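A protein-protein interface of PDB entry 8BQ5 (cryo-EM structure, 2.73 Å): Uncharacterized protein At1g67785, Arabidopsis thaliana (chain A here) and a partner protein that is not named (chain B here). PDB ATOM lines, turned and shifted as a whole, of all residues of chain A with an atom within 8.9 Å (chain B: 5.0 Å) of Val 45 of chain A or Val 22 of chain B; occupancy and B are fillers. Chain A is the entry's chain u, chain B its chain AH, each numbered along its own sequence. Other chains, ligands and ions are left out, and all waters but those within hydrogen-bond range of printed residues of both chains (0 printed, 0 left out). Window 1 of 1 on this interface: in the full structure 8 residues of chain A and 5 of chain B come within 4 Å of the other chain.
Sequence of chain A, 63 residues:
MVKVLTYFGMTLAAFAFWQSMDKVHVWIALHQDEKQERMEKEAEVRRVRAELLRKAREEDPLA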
ATOM      1  N   ARG A  38       0.584   1.316  -8.451  1.00  0.00           N
ATOM      2  CA  ARG A  38      -0.301   2.236  -7.747  1.00  0.00           C
ATOM      3  C   ARG A  38       0.264   2.595  -6.378  1.00  0.00           C
ATOM      4  O   ARG A  38       0.221   3.761  -5.962  1.00  0.00           O
ATOM      5  CB  ARG A  38      -1.687   1.603  -7.627  1.00  0.00           C
ATOM      6  CG  ARG A  38      -2.735   2.450  -6.936  1.00  0.00           C
ATOM      7  CD  ARG A  38      -4.078   1.739  -6.948  1.00  0.00           C
ATOM      8  NE  ARG A  38      -5.129   2.530  -6.311  1.00  0.00           N
ATOM      9  CZ  ARG A  38      -6.422   2.241  -6.348  1.00  0.00           C
ATOM     10  NH1 ARG A  38      -6.882   1.189  -7.004  1.00  0.00           N
ATOM     11  NH2 ARG A  38      -7.282   3.035  -5.712  1.00  0.00           N
ATOM     12  N   MET A  39       0.816   1.606  -5.673  1.00  0.00           N
ATOM     13  CA  MET A  39       1.444   1.860  -4.383  1.00  0.00           C
ATOM     14  C   MET A  39       2.611   2.829  -4.519  1.00  0.00           C
ATOM     15  O   MET A  39       2.773   3.737  -3.697  1.00  0.00           O
ATOM     16  CB  MET A  39       1.914   0.543  -3.766  1.00  0.00           C
ATOM     17  CG  MET A  39       0.969  -0.048  -2.736  1.00  0.00           C
ATOM     18  SD  MET A  39       1.286   0.617  -1.092  1.00  0.00           S
ATOM     19  CE  MET A  39       2.695  -0.370  -0.593  1.00  0.00           C
ATOM     20  N   GLU A  40       3.437   2.646  -5.550  1.00  0.00           N
ATOM     21  CA  GLU A  40       4.566   3.544  -5.764  1.00  0.00           C
ATOM     22  C   GLU A  40       4.100   4.959  -6.070  1.00  0.00           C
ATOM     23  O   GLU A  40       4.665   5.927  -5.549  1.00  0.00           O
ATOM     24  CB  GLU A  40       5.456   3.025  -6.893  1.00  0.00           C
ATOM     25  CG  GLU A  40       6.247   1.791  -6.530  1.00  0.00           C
ATOM     26  CD  GLU A  40       7.100   1.996  -5.297  1.00  0.00           C
ATOM     27  OE1 GLU A  40       7.731   3.068  -5.175  1.00  0.00           O
ATOM     28  OE2 GLU A  40       7.133   1.085  -4.444  1.00  0.00           O
ATOM     29  N   LYS A  41       3.082   5.104  -6.920  1.00  0.00           N
ATOM     30  CA  LYS A  41       2.603   6.443  -7.245  1.00  0.00           C
ATOM     31  C   LYS A  41       2.049   7.138  -6.007  1.00  0.00           C
ATOM     32  O   LYS A  41       2.325   8.322  -5.774  1.00  0.00           O
ATOM     33  CB  LYS A  41       1.550   6.380  -8.351  1.00  0.00           C
ATOM     34  CG  LYS A  41       0.832   7.700  -8.599  1.00  0.00           C
ATOM     35  CD  LYS A  41      -0.455   7.497  -9.385  1.00  0.00           C
ATOM     36  CE  LYS A  41      -1.683   7.749  -8.530  1.00  0.00           C
ATOM     37  NZ  LYS A  41      -2.947   7.545  -9.289  1.00  0.00           N
ATOM     38  N   GLU A  42       1.293   6.410  -5.181  1.00  0.00           N
ATOM     39  CA  GLU A  42       0.736   7.014  -3.975  1.00  0.00           C
ATOM     40  C   GLU A  42       1.827   7.355  -2.960  1.00  0.00           C
ATOM     41  O   GLU A  42       1.754   8.391  -2.283  1.00  0.00           O
ATOM     42  CB  GLU A  42      -0.315   6.080  -3.371  1.00  0.00           C
ATOM     43  CG  GLU A  42      -1.766   6.442  -3.721  1.00  0.00           C
ATOM     44  CD  GLU A  42      -2.092   6.366  -5.213  1.00  0.00           C
ATOM     45  OE1 GLU A  42      -3.240   6.691  -5.586  1.00  0.00           O
ATOM     46  OE2 GLU A  42      -1.224   5.972  -6.017  1.00  0.00           O
ATOM     47  N   ALA A  43       2.847   6.500  -2.841  1.00  0.00           N
ATOM     48  CA  ALA A  43       3.966   6.811  -1.958  1.00  0.00           C
ATOM     49  C   ALA A  43       4.706   8.053  -2.430  1.00  0.00           C
ATOM     50  O   ALA A  43       5.116   8.888  -1.617  1.00  0.00           O
ATOM     51  CB  ALA A  43       4.921   5.620  -1.874  1.00  0.00           C
ATOM     52  N   GLU A  44       4.892   8.184  -3.746  1.00  0.00           N
ATOM     53  CA  GLU A  44       5.520   9.381  -4.291  1.00  0.00           C
ATOM     54  C   GLU A  44       4.679  10.619  -4.010  1.00  0.00           C
ATOM     55  O   GLU A  44       5.218  11.689  -3.710  1.00  0.00           O
ATOM     56  CB  GLU A  44       5.765   9.215  -5.796  1.00  0.00           C
ATOM     57  CG  GLU A  44       6.327  10.441  -6.578  1.00  0.00           C
ATOM     58  CD  GLU A  44       7.518  11.158  -5.924  1.00  0.00           C
ATOM     59  OE1 GLU A  44       8.237  11.885  -6.636  1.00  0.00           O
ATOM     60  OE2 GLU A  44       7.757  11.023  -4.709  1.00  0.00           O
ATOM     61  N   VAL A  45       3.355  10.492  -4.109  1.00  0.00           N
ATOM     62  CA  VAL A  45       2.476  11.611  -3.780  1.00  0.00           C
ATOM     63  C   VAL A  45       2.685  12.039  -2.333  1.00  0.00           C
ATOM     64  O   VAL A  45       2.876  13.228  -2.037  1.00  0.00           O
ATOM     65  CB  VAL A  45       1.008  11.239  -4.048  1.00  0.00           C
ATOM     66  CG1 VAL A  45       0.083  12.291  -3.462  1.00  0.00           C
ATOM     67  CG2 VAL A  45       0.763  11.089  -5.537  1.00  0.00           C
ATOM     68  N   ARG A  46       2.662  11.073  -1.411  1.00  0.00           N
ATOM     69  CA  ARG A  46       2.841  11.403   0.002  1.00  0.00           C
ATOM     70  C   ARG A  46       4.205  12.035   0.255  1.00  0.00           C
ATOM     71  O   ARG A  46       4.319  13.003   1.017  1.00  0.00           O
ATOM     72  CB  ARG A  46       2.671  10.156   0.868  1.00  0.00           C
ATOM     73  CG  ARG A  46       2.816  10.401   2.370  1.00  0.00           C
ATOM     74  CD  ARG A  46       2.563   9.134   3.180  1.00  0.00           C
ATOM     75  NE  ARG A  46       2.677   9.364   4.616  1.00  0.00           N
ATOM     76  CZ  ARG A  46       2.324   8.489   5.548  1.00  0.00           C
ATOM     77  NH1 ARG A  46       1.856   7.294   5.231  1.00  0.00           N
ATOM     78  NH2 ARG A  46       2.458   8.814   6.831  1.00  0.00           N
ATOM     79  N   ARG A  47       5.253  11.500  -0.376  1.00  0.00           N
ATOM     80  CA  ARG A  47       6.601  12.004  -0.137  1.00  0.00           C
ATOM     81  C   ARG A  47       6.772  13.414  -0.689  1.00  0.00           C
ATOM     82  O   ARG A  47       7.394  14.266  -0.044  1.00  0.00           O
ATOM     83  CB  ARG A  47       7.624  11.048  -0.747  1.00  0.00           C
ATOM     84  CG  ARG A  47       9.037  11.193  -0.203  1.00  0.00           C
ATOM     85  CD  ARG A  47       9.974  11.790  -1.241  1.00  0.00           C
ATOM     86  NE  ARG A  47       9.749  11.229  -2.569  1.00  0.00           N
ATOM     87  CZ  ARG A  47      10.140  10.022  -2.956  1.00  0.00           C
ATOM     88  NH1 ARG A  47      10.785   9.208  -2.137  1.00  0.00           N
ATOM     89  NH2 ARG A  47       9.872   9.620  -4.195  1.00  0.00           N
ATOM     90  N   VAL A  48       6.223  13.682  -1.876  1.00  0.00           N
ATOM     91  CA  VAL A  48       6.269  15.029  -2.436  1.00  0.00           C
ATOM     92  C   VAL A  48       5.505  15.998  -1.544  1.00  0.00           C
ATOM     93  O   VAL A  48       5.959  17.122  -1.289  1.00  0.00           O
ATOM     94  CB  VAL A  48       5.722  15.026  -3.875  1.00  0.00           C
ATOM     95  CG1 VAL A  48       5.393  16.441  -4.336  1.00  0.00           C
ATOM     96  CG2 VAL A  48       6.723  14.373  -4.817  1.00  0.00           C
ATOM     97  N   ARG A  49       4.337  15.581  -1.048  1.00  0.00           N
ATOM     98  CA  ARG A  49       3.562  16.454  -0.173  1.00  0.00           C
ATOM     99  C   ARG A  49       4.316  16.759   1.113  1.00  0.00           C
ATOM    100  O   ARG A  49       4.297  17.897   1.598  1.00  0.00           O
ATOM    101  CB  ARG A  49       2.212  15.818   0.145  1.00  0.00           C
ATOM    102  CG  ARG A  49       1.765  16.024   1.580  1.00  0.00           C
ATOM    103  CD  ARG A  49       0.507  15.257   1.899  1.00  0.00           C
ATOM    104  NE  ARG A  49      -0.585  15.567   0.984  1.00  0.00           N
ATOM    105  CZ  ARG A  49      -0.917  14.831  -0.068  1.00  0.00           C
ATOM    106  NH1 ARG A  49      -0.255  13.727  -0.375  1.00  0.00           N
ATOM    107  NH2 ARG A  49      -1.938  15.211  -0.831  1.00  0.00           N
ATOM    108  N   ALA A  50       4.970  15.750   1.690  1.00  0.00           N
ATOM    109  CA  ALA A  50       5.729  15.973   2.914  1.00  0.00           C
ATOM    110  C   ALA A  50       6.921  16.887   2.662  1.00  0.00           C
ATOM    111  O   ALA A  50       7.188  17.802   3.449  1.00  0.00           O
ATOM    112  CB  ALA A  50       6.188  14.636   3.497  1.00  0.00           C
ATOM    113  N   GLU A  51       7.642  16.662   1.563  1.00  0.00           N
ATOM    114  CA  GLU A  51       8.817  17.474   1.277  1.00  0.00           C
ATOM    115  C   GLU A  51       8.427  18.918   0.990  1.00  0.00           C
ATOM    116  O   GLU A  51       9.180  19.845   1.310  1.00  0.00           O
ATOM    117  CB  GLU A  51       9.605  16.855   0.115  1.00  0.00           C
ATOM    118  CG  GLU A  51       8.890  16.784  -1.232  1.00  0.00           C
ATOM    119  CD  GLU A  51       9.699  16.049  -2.285  1.00  0.00           C
ATOM    120  OE1 GLU A  51      10.922  15.900  -2.090  1.00  0.00           O
ATOM    121  OE2 GLU A  51       9.115  15.624  -3.303  1.00  0.00           O
ATOM    122  N   LEU A  52       7.252  19.132   0.394  1.00  0.00           N
ATOM    123  CA  LEU A  52       6.790  20.491   0.143  1.00  0.00           C
ATOM    124  C   LEU A  52       6.270  21.137   1.422  1.00  0.00           C
ATOM    125  O   LEU A  52       6.396  22.353   1.608  1.00  0.00           O
ATOM    126  CB  LEU A  52       5.712  20.477  -0.939  1.00  0.00           C
ATOM    127  CG  LEU A  52       5.815  21.533  -2.039  1.00  0.00           C
ATOM    128  CD1 LEU A  52       7.172  21.468  -2.718  1.00  0.00           C
ATOM    129  CD2 LEU A  52       4.706  21.335  -3.052  1.00  0.00           C
ATOM    130  N   LEU A  53       5.673  20.338   2.310  1.00  0.00           N
ATOM    131  CA  LEU A  53       5.202  20.860   3.589  1.00  0.00           C
ATOM    132  C   LEU A  53       6.350  21.063   4.571  1.00  0.00           C
ATOM    133  O   LEU A  53       6.301  21.986   5.394  1.00  0.00           O
ATOM    134  CB  LEU A  53       4.152  19.920   4.179  1.00  0.00           C
ATOM    135  CG  LEU A  53       3.161  20.495   5.192  1.00  0.00           C
ATOM    136  CD1 LEU A  53       2.088  21.329   4.504  1.00  0.00           C
ATOM    137  CD2 LEU A  53       2.533  19.369   6.000  1.00  0.00           C
ATOM    138  N   LYS B  18      -0.053  24.393  -2.785  1.00  0.00           N
ATOM    139  CA  LYS B  18       0.466  23.243  -3.521  1.00  0.00           C
ATOM    140  C   LYS B  18       0.388  21.928  -2.749  1.00  0.00           C
ATOM    141  O   LYS B  18       0.022  20.912  -3.364  1.00  0.00           O
ATOM    142  CB  LYS B  18       1.902  23.540  -3.971  1.00  0.00           C
ATOM    143  CG  LYS B  18       1.989  24.666  -4.990  1.00  0.00           C
ATOM    144  CD  LYS B  18       3.423  25.004  -5.347  1.00  0.00           C
ATOM    145  CE  LYS B  18       4.085  23.874  -6.112  1.00  0.00           C
ATOM    146  NZ  LYS B  18       5.414  24.280  -6.646  1.00  0.00           N
ATOM    147  N   PRO B  19       0.708  21.857  -1.450  1.00  0.00           N
ATOM    148  CA  PRO B  19       0.588  20.568  -0.747  1.00  0.00           C
ATOM    149  C   PRO B  19      -0.824  20.003  -0.720  1.00  0.00           C
ATOM    150  O   PRO B  19      -0.984  18.802  -0.475  1.00  0.00           O
ATOM    151  CB  PRO B  19       1.093  20.885   0.669  1.00  0.00           C
ATOM    152  CG  PRO B  19       1.069  22.370   0.773  1.00  0.00           C
ATOM    153  CD  PRO B  19       1.373  22.859  -0.599  1.00  0.00           C
ATOM    154  N   LYS B  20      -1.850  20.821  -0.952  1.00  0.00           N
ATOM    155  CA  LYS B  20      -3.206  20.307  -1.093  1.00  0.00           C
ATOM    156  C   LYS B  20      -3.500  19.786  -2.495  1.00  0.00           C
ATOM    157  O   LYS B  20      -4.487  19.065  -2.676  1.00  0.00           O
ATOM    158  CB  LYS B  20      -4.221  21.393  -0.731  1.00  0.00           C
ATOM    159  CG  LYS B  20      -5.671  20.944  -0.775  1.00  0.00           C
ATOM    160  CD  LYS B  20      -6.605  22.069  -0.355  1.00  0.00           C
ATOM    161  CE  LYS B  20      -8.055  21.632  -0.421  1.00  0.00           C
ATOM    162  NZ  LYS B  20      -8.988  22.719  -0.013  1.00  0.00           N
ATOM    163  N   CYS B  21      -2.674  20.119  -3.480  1.00  0.00           N
ATOM    164  CA  CYS B  21      -2.874  19.693  -4.860  1.00  0.00           C
ATOM    165  C   CYS B  21      -1.657  18.936  -5.373  1.00  0.00           C
ATOM    166  O   CYS B  21      -1.254  19.080  -6.528  1.00  0.00           O
ATOM    167  CB  CYS B  21      -3.184  20.886  -5.758  1.00  0.00           C
ATOM    168  SG  CYS B  21      -4.534  21.918  -5.167  1.00  0.00           S
ATOM    169  N   VAL B  22      -1.058  18.114  -4.510  1.00  0.00           N
ATOM    170  CA  VAL B  22       0.140  17.377  -4.895  1.00  0.00           C
ATOM    171  C   VAL B  22      -0.183  16.348  -5.972  1.00  0.00           C
ATOM    172  O   VAL B  22       0.591  16.154  -6.916  1.00  0.00           O
ATOM    173  CB  VAL B  22       0.783  16.729  -3.657  1.00  0.00           C
ATOM    174  CG1 VAL B  22       1.731  15.614  -4.061  1.00  0.00           C
ATOM    175  CG2 VAL B  22       1.515  17.777  -2.843  1.00  0.00           C
ATOM    176  N   LYS B  23      -1.329  15.678  -5.854  1.00  0.00           N
ATOM    177  CA  LYS B  23      -1.696  14.663  -6.840  1.00  0.00           C
ATOM    178  C   LYS B  23      -1.852  15.219  -8.250  1.00  0.00           C
ATOM    179  O   LYS B  23      -1.292  14.620  -9.185  1.00  0.00           O
ATOM    180  CB  LYS B  23      -2.959  13.928  -6.379  1.00  0.00           C
ATOM    181  CG  LYS B  23      -3.011  12.478  -6.827  1.00  0.00           C
ATOM    182  CD  LYS B  23      -3.462  11.551  -5.715  1.00  0.00           C
ATOM    183  CE  LYS B  23      -2.960  10.134  -5.957  1.00  0.00           C
ATOM    184  NZ  LYS B  23      -3.083   9.281  -4.747  1.00  0.00           N
ATOM    185  N   PRO B  24      -2.585  16.314  -8.494  1.00  0.00           N
ATOM    186  CA  PRO B  24      -2.651  16.832  -9.872  1.00  0.00           C
ATOM    187  C   PRO B  24      -1.332  17.386 -10.375  1.00  0.00           C
ATOM    188  O   PRO B  24      -1.029  17.247 -11.567  1.00  0.00           O
ATOM    189  CB  PRO B  24      -3.727  17.925  -9.795  1.00  0.00           C
ATOM    190  CG  PRO B  24      -4.443  17.695  -8.519  1.00  0.00           C
ATOM    191  CD  PRO B  24      -3.457  17.084  -7.591  1.00  0.00           C
ATOM    192  N   LEU B  25      -0.538  18.013  -9.504  1.00  0.00           N
ATOM    193  CA  LEU B  25       0.748  18.558  -9.930  1.00  0.00           C
ATOM    194  C   LEU B  25       1.664  17.459 -10.452  1.00  0.00           C
ATOM    195  O   LEU B  25       2.337  17.631 -11.474  1.00  0.00           O
ATOM    196  CB  LEU B  25       1.408  19.309  -8.774  1.00  0.00           C
ATOM    197  CG  LEU B  25       2.801  19.876  -9.052  1.00  0.00           C
ATOM    198  CD1 LEU B  25       2.771  20.924 -10.150  1.00  0.00           C
ATOM    199  CD2 LEU B  25       3.382  20.460  -7.776  1.00  0.00           C
ATOM    200  N   LEU B  26       1.703  16.320  -9.759  1.00  0.00           N
ATOM    201  CA  LEU B  26       2.533  15.211 -10.217  1.00  0.00           C
ATOM    202  C   LEU B  26       2.037  14.669 -11.551  1.00  0.00           C
ATOM    203  O   LEU B  26       2.839  14.327 -12.427  1.00  0.00           O
ATOM    204  CB  LEU B  26       2.563  14.104  -9.165  1.00  0.00           C
ATOM    205  CG  LEU B  26       3.449  14.369  -7.947  1.00  0.00           C
ATOM    206  CD1 LEU B  26       3.486  13.154  -7.041  1.00  0.00           C
ATOM    207  CD2 LEU B  26       4.852  14.764  -8.373  1.00  0.00           C
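The side-chain carboxylate of Glu 42 of chain A is in salt-bridge range of the side-chain amino group of Lys 23 of chain B (2.7 Å).
The backbone carbonyl oxygen (O) of Arg 38 of chain A sits close to the side-chain carboxylate (OE2) of Glu 42 of chain A.
NZ of Lys 41 of chain A is in salt-bridge range of OE1 of Glu 42 of chain A.
NH2 of Arg 47 of chain A lies within salt-bridge range of OE2 of Glu 44 of chain A (2.6 Å).
Among the printed residues, merely in contact across the chains: Lys 41 of chain A with Lys 23 of chain B, Glu 44 of chain A with Leu 26 of chain B, Val 45 of chain A with Val 22 of chain B, Val 45 of chain A with Lys 23 of chain B, Val 45 of chain A with Leu 26 of chain B, Val 48 of chain A with Val 22 of chain B, Arg 49 of chain A with Pro 19 of chain B, Arg 49 of chain A with Val 22 of chain B, Leu 52 of chain A with Lys 18 of chain B and Leu 53 of chain A with Pro 19 of chain B.
Printed residues of chain B within 4 Å of Lys 41 of chain A: Lys 23.
Of the printed residues of chain B, Glu 42 of chain A touches Lys 23.
Of the printed residues of chain B, Glu 44 of chain A touches Leu 26.
Val 45 of chain A touches just these residues of chain B: Val 22, Lys 23 and Leu 26.
Of the printed residues of chain B, Leu 53 of chain A touches Pro 19 (3.99 Å).
Of chain A, only Val 45, Val 48 and Arg 49 come within 4 Å of Val 22 of chain B.
Lys 23 of chain B touches just these residues of chain A: Lys 41, Glu 42 and Val 45.
The nearest printed residue of chain B that does not touch Leu 53 of chain A is Lys 20 of chain B (6.7 Å).
Hydrophobic or aromatic side chains of chain A that line the printed part of chain B: Val 45, Val 48, Leu 52 and Leu 53.
Along chain A the printed residues that touch a printed residue of chain B span positions 41 to 53.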
